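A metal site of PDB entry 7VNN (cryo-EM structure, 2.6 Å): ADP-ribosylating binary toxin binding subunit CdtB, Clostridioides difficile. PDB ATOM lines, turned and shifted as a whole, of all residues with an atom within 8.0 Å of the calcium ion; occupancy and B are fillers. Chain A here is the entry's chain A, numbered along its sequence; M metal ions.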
ATOM      1  N   CYS A 374     -18.236   7.792   8.428  1.00  0.00           N
ATOM      2  CA  CYS A 374     -19.237   8.007   7.384  1.00  0.00           C
ATOM      3  C   CYS A 374     -18.858   7.356   6.074  1.00  0.00           C
ATOM      4  O   CYS A 374     -19.581   7.529   5.077  1.00  0.00           O
ATOM      5  CB  CYS A 374     -19.469   9.506   7.192  1.00  0.00           C
ATOM      6  SG  CYS A 374     -19.850  10.408   8.709  1.00  0.00           S
ATOM      7  N   PHE A 418     -26.607   7.425   2.471  1.00  0.00           N
ATOM      8  CA  PHE A 418     -26.106   7.579   3.816  1.00  0.00           C
ATOM      9  C   PHE A 418     -26.969   8.576   4.575  1.00  0.00           C
ATOM     10  O   PHE A 418     -27.415   9.572   4.000  1.00  0.00           O
ATOM     11  CB  PHE A 418     -24.639   8.054   3.817  1.00  0.00           C
ATOM     12  CG  PHE A 418     -24.089   8.328   5.178  1.00  0.00           C
ATOM     13  CD1 PHE A 418     -23.757   7.299   6.035  1.00  0.00           C
ATOM     14  CD2 PHE A 418     -23.897   9.637   5.612  1.00  0.00           C
ATOM     15  CE1 PHE A 418     -23.241   7.554   7.290  1.00  0.00           C
ATOM     16  CE2 PHE A 418     -23.388   9.898   6.864  1.00  0.00           C
ATOM     17  CZ  PHE A 418     -23.060   8.857   7.703  1.00  0.00           C
ATOM     18  N   THR A 419     -27.208   8.293   5.847  1.00  0.00           N
ATOM     19  CA  THR A 419     -27.934   9.209   6.716  1.00  0.00           C
ATOM     20  C   THR A 419     -27.270   9.275   8.076  1.00  0.00           C
ATOM     21  O   THR A 419     -26.816   8.259   8.613  1.00  0.00           O
ATOM     22  CB  THR A 419     -29.409   8.786   6.869  1.00  0.00           C
ATOM     23  OG1 THR A 419     -30.062   9.667   7.791  1.00  0.00           O
ATOM     24  CG2 THR A 419     -29.519   7.356   7.367  1.00  0.00           C
ATOM     25  N   ASN A 420     -27.171  10.491   8.618  1.00  0.00           N
ATOM     26  CA  ASN A 420     -26.703  10.708   9.976  1.00  0.00           C
ATOM     27  C   ASN A 420     -27.773  11.321  10.868  1.00  0.00           C
ATOM     28  O   ASN A 420     -27.491  11.622  12.031  1.00  0.00           O
ATOM     29  CB  ASN A 420     -25.459  11.602   9.973  1.00  0.00           C
ATOM     30  CG  ASN A 420     -25.721  12.954   9.351  1.00  0.00           C
ATOM     31  OD1 ASN A 420     -26.737  13.152   8.685  1.00  0.00           O
ATOM     32  ND2 ASN A 420     -24.808  13.891   9.557  1.00  0.00           N
ATOM     33  N   PHE A 421     -28.983  11.526  10.345  1.00  0.00           N
ATOM     34  CA  PHE A 421     -30.115  12.118  11.054  1.00  0.00           C
ATOM     35  C   PHE A 421     -29.828  13.533  11.525  1.00  0.00           C
ATOM     36  O   PHE A 421     -30.514  14.050  12.410  1.00  0.00           O
ATOM     37  CB  PHE A 421     -30.547  11.246  12.248  1.00  0.00           C
ATOM     38  CG  PHE A 421     -30.592   9.774  11.940  1.00  0.00           C
ATOM     39  CD1 PHE A 421     -31.540   9.269  11.079  1.00  0.00           C
ATOM     40  CD2 PHE A 421     -29.700   8.914  12.543  1.00  0.00           C
ATOM     41  CE1 PHE A 421     -31.579   7.919  10.800  1.00  0.00           C
ATOM     42  CE2 PHE A 421     -29.748   7.558  12.281  1.00  0.00           C
ATOM     43  CZ  PHE A 421     -30.687   7.058  11.404  1.00  0.00           C
ATOM     44  N   ASP A 422     -28.814  14.186  10.964  1.00  0.00           N
ATOM     45  CA  ASP A 422     -28.475  15.553  11.319  1.00  0.00           C
ATOM     46  C   ASP A 422     -28.681  16.520  10.157  1.00  0.00           C
ATOM     47  O   ASP A 422     -29.454  17.474  10.277  1.00  0.00           O
ATOM     48  CB  ASP A 422     -27.020  15.616  11.800  1.00  0.00           C
ATOM     49  CG  ASP A 422     -26.714  14.588  12.868  1.00  0.00           C
ATOM     50  OD1 ASP A 422     -27.638  14.212  13.614  1.00  0.00           O
ATOM     51  OD2 ASP A 422     -25.555  14.131  12.940  1.00  0.00           O
ATOM     52  N   ASP A 423     -28.003  16.286   9.037  1.00  0.00           N
ATOM     53  CA  ASP A 423     -28.164  17.119   7.858  1.00  0.00           C
ATOM     54  C   ASP A 423     -28.084  16.333   6.553  1.00  0.00           C
ATOM     55  O   ASP A 423     -28.270  16.925   5.487  1.00  0.00           O
ATOM     56  CB  ASP A 423     -27.110  18.233   7.842  1.00  0.00           C
ATOM     57  CG  ASP A 423     -25.693  17.708   7.999  1.00  0.00           C
ATOM     58  OD1 ASP A 423     -25.536  16.495   8.263  1.00  0.00           O
ATOM     59  OD2 ASP A 423     -24.739  18.503   7.852  1.00  0.00           O
ATOM     60  N   THR A 436     -35.164  11.965  16.602  1.00  0.00           N
ATOM     61  CA  THR A 436     -34.041  12.888  16.600  1.00  0.00           C
ATOM     62  C   THR A 436     -34.310  14.049  17.561  1.00  0.00           C
ATOM     63  O   THR A 436     -34.187  15.225  17.227  1.00  0.00           O
ATOM     64  CB  THR A 436     -33.766  13.377  15.175  1.00  0.00           C
ATOM     65  OG1 THR A 436     -33.652  12.241  14.313  1.00  0.00           O
ATOM     66  CG2 THR A 436     -32.437  14.133  15.105  1.00  0.00           C
ATOM     67  N   ASP A 440     -27.751  12.145  21.389  1.00  0.00           N
ATOM     68  CA  ASP A 440     -27.086  10.861  21.556  1.00  0.00           C
ATOM     69  C   ASP A 440     -26.605  10.371  20.188  1.00  0.00           C
ATOM     70  O   ASP A 440     -26.992  10.895  19.142  1.00  0.00           O
ATOM     71  CB  ASP A 440     -28.014   9.835  22.214  1.00  0.00           C
ATOM     72  CG  ASP A 440     -28.402  10.229  23.628  1.00  0.00           C
ATOM     73  OD1 ASP A 440     -27.505  10.628  24.392  1.00  0.00           O
ATOM     74  OD2 ASP A 440     -29.594  10.148  23.962  1.00  0.00           O
ATOM     75  N   GLY A 441     -25.735   9.364  20.211  1.00  0.00           N
ATOM     76  CA  GLY A 441     -25.116   8.891  18.984  1.00  0.00           C
ATOM     77  C   GLY A 441     -23.745   9.491  18.769  1.00  0.00           C
ATOM     78  O   GLY A 441     -23.199  10.220  19.596  1.00  0.00           O
ATOM     79  N   LEU A 442     -23.177   9.164  17.606  1.00  0.00           N
ATOM     80  CA  LEU A 442     -21.879   9.727  17.245  1.00  0.00           C
ATOM     81  C   LEU A 442     -21.942  11.240  17.127  1.00  0.00           C
ATOM     82  O   LEU A 442     -21.039  11.945  17.587  1.00  0.00           O
ATOM     83  CB  LEU A 442     -21.371   9.108  15.934  1.00  0.00           C
ATOM     84  CG  LEU A 442     -20.655   7.751  15.964  1.00  0.00           C
ATOM     85  CD1 LEU A 442     -19.360   7.851  16.759  1.00  0.00           C
ATOM     86  CD2 LEU A 442     -21.538   6.632  16.500  1.00  0.00           C
ATOM     87  N   GLN A 443     -23.010  11.763  16.510  1.00  0.00           N
ATOM     88  CA  GLN A 443     -23.240  13.201  16.454  1.00  0.00           C
ATOM     89  C   GLN A 443     -24.742  13.443  16.576  1.00  0.00           C
ATOM     90  O   GLN A 443     -25.438  13.508  15.559  1.00  0.00           O
ATOM     91  CB  GLN A 443     -22.678  13.802  15.176  1.00  0.00           C
ATOM     92  CG  GLN A 443     -21.160  13.935  15.133  1.00  0.00           C
ATOM     93  CD  GLN A 443     -20.482  12.725  14.525  1.00  0.00           C
ATOM     94  OE1 GLN A 443     -21.019  12.078  13.622  1.00  0.00           O
ATOM     95  NE2 GLN A 443     -19.285  12.404  15.016  1.00  0.00           N
ATOM     96  N   GLY A 444     -25.223  13.572  17.807  1.00  0.00           N
ATOM     97  CA  GLY A 444     -26.598  13.948  18.100  1.00  0.00           C
ATOM     98  C   GLY A 444     -27.694  13.322  17.251  1.00  0.00           C
ATOM     99  O   GLY A 444     -28.410  14.030  16.543  1.00  0.00           O
ATOM    100  N   SER A 445     -27.841  12.004  17.313  1.00  0.00           N
ATOM    101  CA  SER A 445     -28.875  11.321  16.539  1.00  0.00           C
ATOM    102  C   SER A 445     -29.063   9.908  17.082  1.00  0.00           C
ATOM    103  O   SER A 445     -28.086   9.173  17.262  1.00  0.00           O
ATOM    104  CB  SER A 445     -28.498  11.270  15.048  1.00  0.00           C
ATOM    105  OG  SER A 445     -27.338  10.479  14.839  1.00  0.00           O
ATOM    106  N   ALA A 446     -30.316   9.530  17.337  1.00  0.00           N
ATOM    107  CA  ALA A 446     -30.626   8.217  17.892  1.00  0.00           C
ATOM    108  C   ALA A 446     -31.457   7.356  16.949  1.00  0.00           C
ATOM    109  O   ALA A 446     -31.025   6.263  16.585  1.00  0.00           O
ATOM    110  CB  ALA A 446     -31.359   8.399  19.226  1.00  0.00           C
ATOM    111  N   LEU A 532     -29.005   3.694  17.194  1.00  0.00           N
ATOM    112  CA  LEU A 532     -28.431   3.462  15.875  1.00  0.00           C
ATOM    113  C   LEU A 532     -27.928   4.792  15.326  1.00  0.00           C
ATOM    114  O   LEU A 532     -28.426   5.858  15.668  1.00  0.00           O
ATOM    115  CB  LEU A 532     -29.447   2.841  14.905  1.00  0.00           C
ATOM    116  CG  LEU A 532     -29.958   1.439  15.261  1.00  0.00           C
ATOM    117  CD1 LEU A 532     -30.977   0.975  14.232  1.00  0.00           C
ATOM    118  CD2 LEU A 532     -28.808   0.457  15.365  1.00  0.00           C
ATOM    119  N   ASP A 533     -26.924   4.709  14.445  1.00  0.00           N
ATOM    120  CA  ASP A 533     -26.346   5.907  13.872  1.00  0.00           C
ATOM    121  C   ASP A 533     -25.565   5.561  12.608  1.00  0.00           C
ATOM    122  O   ASP A 533     -24.957   4.492  12.527  1.00  0.00           O
ATOM    123  CB  ASP A 533     -25.421   6.610  14.877  1.00  0.00           C
ATOM    124  CG  ASP A 533     -25.493   8.118  14.776  1.00  0.00           C
ATOM    125  OD1 ASP A 533     -26.294   8.617  13.956  1.00  0.00           O
ATOM    126  OD2 ASP A 533     -24.769   8.804  15.510  1.00  0.00           O
ATOM    127  N   ASN A 534     -25.612   6.475  11.636  1.00  0.00           N
ATOM    128  CA  ASN A 534     -24.804   6.402  10.413  1.00  0.00           C
ATOM    129  C   ASN A 534     -25.076   5.119   9.635  1.00  0.00           C
ATOM    130  O   ASN A 534     -24.206   4.276   9.438  1.00  0.00           O
ATOM    131  CB  ASN A 534     -23.313   6.537  10.747  1.00  0.00           C
ATOM    132  CG  ASN A 534     -22.960   7.891  11.319  1.00  0.00           C
ATOM    133  OD1 ASN A 534     -23.731   8.842  11.214  1.00  0.00           O
ATOM    134  ND2 ASN A 534     -21.785   7.985  11.940  1.00  0.00           N
HETATM  135 CA    CA M   1     -25.558  11.723  13.855  1.00  0.00          CA
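The side-chain carboxylate of Asp 533 lies close to the side-chain hydroxyl of Ser 445.
The side-chain carboxylate (OD2) of Asp 533 lies within hydrogen-bond range of the backbone NH (N) of Leu 442, at 2.7 Å.
The side-chain amide nitrogen of Asn 420 is in hydrogen-bond range of the side-chain carboxylate of Asp 423, 3.0 Å away.
Asp 533 touches the calcium ion (OD1 to CA, 3.2 Å).
The calcium ion is bound by the side-chain hydroxyl of Ser 445 (2.4 Å), the backbone carbonyl oxygen of Gln 443 (2.5 Å), the side-chain carboxylate of Asp 422 (2.6 Å) and the backbone carbonyl oxygen of Asn 420 (2.7 Å).
The calcium ion has four donor atoms within binding distance.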
